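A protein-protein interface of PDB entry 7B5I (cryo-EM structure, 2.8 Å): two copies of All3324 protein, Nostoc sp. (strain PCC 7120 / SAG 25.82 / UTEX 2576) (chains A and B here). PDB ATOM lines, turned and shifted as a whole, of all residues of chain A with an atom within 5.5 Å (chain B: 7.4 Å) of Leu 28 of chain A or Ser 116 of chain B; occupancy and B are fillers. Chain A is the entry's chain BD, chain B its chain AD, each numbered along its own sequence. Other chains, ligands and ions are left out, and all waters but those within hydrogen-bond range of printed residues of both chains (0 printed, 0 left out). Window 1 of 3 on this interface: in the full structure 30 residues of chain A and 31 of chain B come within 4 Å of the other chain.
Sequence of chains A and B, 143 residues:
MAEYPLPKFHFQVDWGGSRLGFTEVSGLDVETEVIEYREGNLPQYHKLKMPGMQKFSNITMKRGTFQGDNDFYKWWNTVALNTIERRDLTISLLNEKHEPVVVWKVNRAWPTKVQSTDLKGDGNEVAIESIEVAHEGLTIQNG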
ATOM      1  N   VAL A  25       6.071   0.600 -12.172  1.00  0.00           N
ATOM      2  CA  VAL A  25       6.103  -0.026 -13.488  1.00  0.00           C
ATOM      3  C   VAL A  25       4.695  -0.498 -13.826  1.00  0.00           C
ATOM      4  O   VAL A  25       4.154  -1.365 -13.135  1.00  0.00           O
ATOM      5  CB  VAL A  25       7.109  -1.190 -13.537  1.00  0.00           C
ATOM      6  CG1 VAL A  25       6.975  -1.952 -14.834  1.00  0.00           C
ATOM      7  CG2 VAL A  25       8.519  -0.669 -13.394  1.00  0.00           C
ATOM      8  N   SER A  26       4.069   0.106 -14.835  1.00  0.00           N
ATOM      9  CA  SER A  26       2.728  -0.321 -15.214  1.00  0.00           C
ATOM     10  C   SER A  26       2.559  -0.383 -16.728  1.00  0.00           C
ATOM     11  O   SER A  26       3.255   0.300 -17.479  1.00  0.00           O
ATOM     12  CB  SER A  26       1.659   0.601 -14.619  1.00  0.00           C
ATOM     13  OG  SER A  26       1.619   1.844 -15.295  1.00  0.00           O
ATOM     14  N   GLY A  27       1.612  -1.211 -17.168  1.00  0.00           N
ATOM     15  CA  GLY A  27       1.248  -1.276 -18.570  1.00  0.00           C
ATOM     16  C   GLY A  27       1.386  -2.620 -19.258  1.00  0.00           C
ATOM     17  O   GLY A  27       1.529  -2.652 -20.481  1.00  0.00           O
ATOM     18  N   LEU A  28       1.369  -3.725 -18.517  1.00  0.00           N
ATOM     19  CA  LEU A  28       1.720  -5.037 -19.055  1.00  0.00           C
ATOM     20  C   LEU A  28       0.457  -5.810 -19.432  1.00  0.00           C
ATOM     21  O   LEU A  28      -0.146  -6.487 -18.597  1.00  0.00           O
ATOM     22  CB  LEU A  28       2.548  -5.807 -18.034  1.00  0.00           C
ATOM     23  CG  LEU A  28       3.780  -5.076 -17.489  1.00  0.00           C
ATOM     24  CD1 LEU A  28       4.457  -5.889 -16.407  1.00  0.00           C
ATOM     25  CD2 LEU A  28       4.752  -4.749 -18.593  1.00  0.00           C
ATOM     26  N   ASP A  29       0.078  -5.737 -20.710  1.00  0.00           N
ATOM     27  CA  ASP A  29      -1.195  -6.258 -21.204  1.00  0.00           C
ATOM     28  C   ASP A  29      -1.000  -6.880 -22.582  1.00  0.00           C
ATOM     29  O   ASP A  29      -0.021  -6.598 -23.274  1.00  0.00           O
ATOM     30  CB  ASP A  29      -2.269  -5.162 -21.307  1.00  0.00           C
ATOM     31  CG  ASP A  29      -2.738  -4.643 -19.961  1.00  0.00           C
ATOM     32  OD1 ASP A  29      -3.958  -4.433 -19.806  1.00  0.00           O
ATOM     33  OD2 ASP A  29      -1.915  -4.414 -19.060  1.00  0.00           O
ATOM     34  N   VAL A  30      -1.957  -7.727 -22.978  1.00  0.00           N
ATOM     35  CA  VAL A  30      -2.038  -8.302 -24.318  1.00  0.00           C
ATOM     36  C   VAL A  30      -3.508  -8.382 -24.711  1.00  0.00           C
ATOM     37  O   VAL A  30      -4.377  -8.569 -23.856  1.00  0.00           O
ATOM     38  CB  VAL A  30      -1.382  -9.698 -24.390  1.00  0.00           C
ATOM     39  CG1 VAL A  30       0.129  -9.595 -24.300  1.00  0.00           C
ATOM     40  CG2 VAL A  30      -1.905 -10.583 -23.287  1.00  0.00           C
ATOM     41  N   ILE A  59       4.374   1.079 -22.097  1.00  0.00           N
ATOM     42  CA  ILE A  59       4.797   0.780 -20.733  1.00  0.00           C
ATOM     43  C   ILE A  59       5.320   2.052 -20.085  1.00  0.00           C
ATOM     44  O   ILE A  59       6.064   2.814 -20.711  1.00  0.00           O
ATOM     45  CB  ILE A  59       5.849  -0.337 -20.712  1.00  0.00           C
ATOM     46  CG1 ILE A  59       5.247  -1.612 -21.297  1.00  0.00           C
ATOM     47  CG2 ILE A  59       6.337  -0.584 -19.311  1.00  0.00           C
ATOM     48  CD1 ILE A  59       6.227  -2.725 -21.484  1.00  0.00           C
ATOM     49  N   ILE A  91      11.946  -7.462 -17.268  1.00  0.00           N
ATOM     50  CA  ILE A  91      11.384  -7.106 -15.970  1.00  0.00           C
ATOM     51  C   ILE A  91      11.210  -8.389 -15.178  1.00  0.00           C
ATOM     52  O   ILE A  91      10.710  -9.381 -15.714  1.00  0.00           O
ATOM     53  CB  ILE A  91      10.048  -6.358 -16.123  1.00  0.00           C
ATOM     54  CG1 ILE A  91      10.218  -5.189 -17.087  1.00  0.00           C
ATOM     55  CG2 ILE A  91       9.566  -5.840 -14.794  1.00  0.00           C
ATOM     56  CD1 ILE A  91       8.936  -4.649 -17.621  1.00  0.00           C
ATOM     57  N   TRP A 104       8.960 -10.800 -17.508  1.00  0.00           N
ATOM     58  CA  TRP A 104       8.358 -10.196 -18.687  1.00  0.00           C
ATOM     59  C   TRP A 104       9.475  -9.781 -19.634  1.00  0.00           C
ATOM     60  O   TRP A 104      10.385  -9.038 -19.241  1.00  0.00           O
ATOM     61  CB  TRP A 104       7.501  -8.984 -18.318  1.00  0.00           C
ATOM     62  CG  TRP A 104       6.286  -9.295 -17.496  1.00  0.00           C
ATOM     63  CD1 TRP A 104       5.040  -9.584 -17.957  1.00  0.00           C
ATOM     64  CD2 TRP A 104       6.199  -9.316 -16.069  1.00  0.00           C
ATOM     65  NE1 TRP A 104       4.184  -9.795 -16.911  1.00  0.00           N
ATOM     66  CE2 TRP A 104       4.871  -9.636 -15.739  1.00  0.00           C
ATOM     67  CE3 TRP A 104       7.114  -9.099 -15.038  1.00  0.00           C
ATOM     68  CZ2 TRP A 104       4.437  -9.746 -14.423  1.00  0.00           C
ATOM     69  CZ3 TRP A 104       6.682  -9.208 -13.737  1.00  0.00           C
ATOM     70  CH2 TRP A 104       5.357  -9.529 -13.439  1.00  0.00           C
ATOM     71  N   LEU A 138       5.811  -8.770 -26.428  1.00  0.00           N
ATOM     72  CA  LEU A 138       5.824  -9.034 -24.995  1.00  0.00           C
ATOM     73  C   LEU A 138       5.574 -10.514 -24.747  1.00  0.00           C
ATOM     74  O   LEU A 138       4.749 -11.131 -25.420  1.00  0.00           O
ATOM     75  CB  LEU A 138       4.766  -8.203 -24.267  1.00  0.00           C
ATOM     76  CG  LEU A 138       4.633  -8.403 -22.761  1.00  0.00           C
ATOM     77  CD1 LEU A 138       5.950  -8.183 -22.059  1.00  0.00           C
ATOM     78  CD2 LEU A 138       3.581  -7.467 -22.225  1.00  0.00           C
ATOM     79  N   ILE A 140       5.465 -13.589 -21.390  1.00  0.00           N
ATOM     80  CA  ILE A 140       5.403 -13.873 -19.958  1.00  0.00           C
ATOM     81  C   ILE A 140       5.982 -15.254 -19.690  1.00  0.00           C
ATOM     82  O   ILE A 140       5.670 -16.215 -20.401  1.00  0.00           O
ATOM     83  CB  ILE A 140       3.959 -13.798 -19.429  1.00  0.00           C
ATOM     84  CG1 ILE A 140       3.320 -12.463 -19.794  1.00  0.00           C
ATOM     85  CG2 ILE A 140       3.926 -14.006 -17.929  1.00  0.00           C
ATOM     86  CD1 ILE A 140       1.913 -12.326 -19.302  1.00  0.00           C
ATOM     87  N   THR B  65      -1.637 -14.260  -7.740  1.00  0.00           N
ATOM     88  CA  THR B  65      -0.510 -14.833  -8.465  1.00  0.00           C
ATOM     89  C   THR B  65       0.315 -15.760  -7.579  1.00  0.00           C
ATOM     90  O   THR B  65       0.681 -15.405  -6.457  1.00  0.00           O
ATOM     91  CB  THR B  65       0.387 -13.726  -9.014  1.00  0.00           C
ATOM     92  OG1 THR B  65      -0.419 -12.707  -9.612  1.00  0.00           O
ATOM     93  CG2 THR B  65       1.332 -14.287 -10.055  1.00  0.00           C
ATOM     94  N   TYR B  73      -1.996 -17.168 -19.410  1.00  0.00           N
ATOM     95  CA  TYR B  73      -1.148 -16.978 -20.576  1.00  0.00           C
ATOM     96  C   TYR B  73      -1.192 -18.228 -21.444  1.00  0.00           C
ATOM     97  O   TYR B  73      -1.263 -18.130 -22.670  1.00  0.00           O
ATOM     98  CB  TYR B  73       0.290 -16.681 -20.147  1.00  0.00           C
ATOM     99  CG  TYR B  73       1.201 -16.287 -21.286  1.00  0.00           C
ATOM    100  CD1 TYR B  73       1.833 -17.250 -22.062  1.00  0.00           C
ATOM    101  CD2 TYR B  73       1.435 -14.950 -21.584  1.00  0.00           C
ATOM    102  CE1 TYR B  73       2.668 -16.894 -23.104  1.00  0.00           C
ATOM    103  CE2 TYR B  73       2.268 -14.584 -22.623  1.00  0.00           C
ATOM    104  CZ  TYR B  73       2.883 -15.559 -23.380  1.00  0.00           C
ATOM    105  OH  TYR B  73       3.713 -15.200 -24.415  1.00  0.00           O
ATOM    106  N   VAL B 114      -5.726 -10.506 -21.282  1.00  0.00           N
ATOM    107  CA  VAL B 114      -5.028 -10.902 -20.062  1.00  0.00           C
ATOM    108  C   VAL B 114      -4.247  -9.703 -19.548  1.00  0.00           C
ATOM    109  O   VAL B 114      -3.462  -9.109 -20.292  1.00  0.00           O
ATOM    110  CB  VAL B 114      -4.078 -12.093 -20.297  1.00  0.00           C
ATOM    111  CG1 VAL B 114      -3.210 -12.320 -19.082  1.00  0.00           C
ATOM    112  CG2 VAL B 114      -4.854 -13.343 -20.617  1.00  0.00           C
ATOM    113  N   GLN B 115      -4.449  -9.346 -18.283  1.00  0.00           N
ATOM    114  CA  GLN B 115      -3.739  -8.227 -17.676  1.00  0.00           C
ATOM    115  C   GLN B 115      -3.004  -8.676 -16.423  1.00  0.00           C
ATOM    116  O   GLN B 115      -3.596  -9.302 -15.538  1.00  0.00           O
ATOM    117  CB  GLN B 115      -4.690  -7.086 -17.339  1.00  0.00           C
ATOM    118  CG  GLN B 115      -5.443  -6.551 -18.526  1.00  0.00           C
ATOM    119  CD  GLN B 115      -6.477  -5.529 -18.128  1.00  0.00           C
ATOM    120  OE1 GLN B 115      -7.093  -5.643 -17.073  1.00  0.00           O
ATOM    121  NE2 GLN B 115      -6.675  -4.525 -18.969  1.00  0.00           N
ATOM    122  N   SER B 116      -1.721  -8.344 -16.348  1.00  0.00           N
ATOM    123  CA  SER B 116      -0.890  -8.670 -15.203  1.00  0.00           C
ATOM    124  C   SER B 116      -0.879  -7.523 -14.202  1.00  0.00           C
ATOM    125  O   SER B 116      -1.450  -6.455 -14.426  1.00  0.00           O
ATOM    126  CB  SER B 116       0.530  -9.000 -15.650  1.00  0.00           C
ATOM    127  OG  SER B 116       0.541 -10.175 -16.437  1.00  0.00           O
ATOM    128  N   THR B 117      -0.212  -7.755 -13.079  1.00  0.00           N
ATOM    129  CA  THR B 117      -0.214  -6.782 -12.005  1.00  0.00           C
ATOM    130  C   THR B 117       0.713  -5.617 -12.332  1.00  0.00           C
ATOM    131  O   THR B 117       1.507  -5.658 -13.270  1.00  0.00           O
ATOM    132  CB  THR B 117       0.204  -7.429 -10.688  1.00  0.00           C
ATOM    133  OG1 THR B 117       0.199  -6.441  -9.654  1.00  0.00           O
ATOM    134  CG2 THR B 117       1.590  -8.031 -10.803  1.00  0.00           C
ATOM    135  N   ASP B 118       0.589  -4.560 -11.543  1.00  0.00           N
ATOM    136  CA  ASP B 118       1.480  -3.413 -11.591  1.00  0.00           C
ATOM    137  C   ASP B 118       2.407  -3.471 -10.388  1.00  0.00           C
ATOM    138  O   ASP B 118       2.071  -4.066  -9.365  1.00  0.00           O
ATOM    139  CB  ASP B 118       0.695  -2.102 -11.600  1.00  0.00           C
ATOM    140  CG  ASP B 118      -0.192  -1.954 -10.400  1.00  0.00           C
ATOM    141  OD1 ASP B 118      -0.907  -2.920 -10.065  1.00  0.00           O
ATOM    142  OD2 ASP B 118      -0.188  -0.865  -9.786  1.00  0.00           O
ATOM    143  N   LEU B 119       3.580  -2.863 -10.517  1.00  0.00           N
ATOM    144  CA  LEU B 119       4.628  -2.967  -9.513  1.00  0.00           C
ATOM    145  C   LEU B 119       4.822  -1.617  -8.839  1.00  0.00           C
ATOM    146  O   LEU B 119       5.068  -0.615  -9.514  1.00  0.00           O
ATOM    147  CB  LEU B 119       5.929  -3.438 -10.158  1.00  0.00           C
ATOM    148  CG  LEU B 119       5.791  -4.649 -11.081  1.00  0.00           C
ATOM    149  CD1 LEU B 119       6.971  -4.741 -12.016  1.00  0.00           C
ATOM    150  CD2 LEU B 119       5.649  -5.930 -10.288  1.00  0.00           C
ATOM    151  N   ALA B 127      -0.228  -9.329  -5.405  1.00  0.00           N
ATOM    152  CA  ALA B 127      -0.293  -9.151  -6.847  1.00  0.00           C
ATOM    153  C   ALA B 127      -1.483  -9.920  -7.407  1.00  0.00           C
ATOM    154  O   ALA B 127      -1.694 -11.088  -7.071  1.00  0.00           O
ATOM    155  CB  ALA B 127       1.002  -9.618  -7.500  1.00  0.00           C
ATOM    156  N   ILE B 128      -2.288  -9.237  -8.218  1.00  0.00           N
ATOM    157  CA  ILE B 128      -3.484  -9.828  -8.811  1.00  0.00           C
ATOM    158  C   ILE B 128      -3.485  -9.703 -10.334  1.00  0.00           C
ATOM    159  O   ILE B 128      -3.043  -8.697 -10.888  1.00  0.00           O
ATOM    160  CB  ILE B 128      -4.772  -9.167  -8.265  1.00  0.00           C
ATOM    161  CG1 ILE B 128      -4.653  -8.887  -6.764  1.00  0.00           C
ATOM    162  CG2 ILE B 128      -5.991 -10.034  -8.544  1.00  0.00           C
ATOM    163  CD1 ILE B 128      -5.876  -8.225  -6.168  1.00  0.00           C
ATOM    164  N   GLU B 129      -3.989 -10.737 -11.001  1.00  0.00           N
ATOM    165  CA  GLU B 129      -4.077 -10.773 -12.452  1.00  0.00           C
ATOM    166  C   GLU B 129      -5.524 -10.986 -12.878  1.00  0.00           C
ATOM    167  O   GLU B 129      -6.355 -11.494 -12.117  1.00  0.00           O
ATOM    168  CB  GLU B 129      -3.190 -11.875 -13.024  1.00  0.00           C
ATOM    169  CG  GLU B 129      -3.423 -13.220 -12.381  1.00  0.00           C
ATOM    170  CD  GLU B 129      -2.550 -14.291 -12.983  1.00  0.00           C
ATOM    171  OE1 GLU B 129      -1.795 -13.974 -13.923  1.00  0.00           O
ATOM    172  OE2 GLU B 129      -2.623 -15.448 -12.528  1.00  0.00           O
ATOM    173  N   SER B 130      -5.816 -10.600 -14.121  1.00  0.00           N
ATOM    174  CA  SER B 130      -7.183 -10.602 -14.613  1.00  0.00           C
ATOM    175  C   SER B 130      -7.248 -11.207 -16.006  1.00  0.00           C
ATOM    176  O   SER B 130      -6.304 -11.101 -16.793  1.00  0.00           O
ATOM    177  CB  SER B 130      -7.757  -9.184 -14.655  1.00  0.00           C
ATOM    178  OG  SER B 130      -7.589  -8.540 -13.411  1.00  0.00           O
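Hydrophobic or aromatic side chains of chain B that line the printed part of chain A: Tyr 73, Val 114 and Leu 119.
Among the printed residues, no Asp or Glu carboxylate lies within 4 Å of a Lys or Arg side-chain nitrogen of the other chain.
Among the printed residues, merely in contact across the chains: Ile 140 of chain A with Tyr 73 of chain B (3.5 Å), Trp 104 of chain A with Ser 116 of chain B (3.7 Å), Val 25 of chain A with Asp 118 of chain B (3.7 Å), Asp 29 of chain A with Val 114 of chain B (3.8 Å), Ile 140 of chain A with Ser 116 of chain B (3.8 Å) and Ile 91 of chain A with Leu 119 of chain B (3.96 Å).
No residue of chain B comes within 4 Å of Gly 27 of chain A.
Leu 28 of chain A touches one residue of chain B.
Printed residues of chain B within 4 Å of Val 30 of chain A: Val 114.
Ile 59 of chain A touches none of the printed residues of chain B.
Of the printed residues of chain B, Trp 104 of chain A touches Ser 116.
Ala 127 of chain B touches none of the printed residues of chain A.
The nearest residue of chain A that does not touch Ser 116 of chain B is Asp 29 of chain A (4.8 Å).
No position is printed for both chains.
The backbone carbonyl oxygen of Val 114 of chain B is in hydrogen-bond range of the backbone NH of Val 30 of chain A (3.4 Å).
The side-chain amide nitrogen (NE2) of Gln 115 of chain B sits at hydrogen-bond distance from the side-chain carboxylate (OD1) of Asp 29 of chain A (2.8 Å).
The backbone NH of Ser 116 of chain B is in hydrogen-bond range of the backbone carbonyl oxygen of Leu 28 of chain A (3.3 Å).
N of Leu 119 of chain B is in hydrogen-bond range of O of Val 25 of chain A, at 3.1 Å.
O of Gln 115 of chain B sits at hydrogen-bond distance from N of Ser 130 of chain B (2.9 Å).
O of Ile 91 of chain A sits at hydrogen-bond distance from N of Trp 104 of chain A (2.9 Å).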
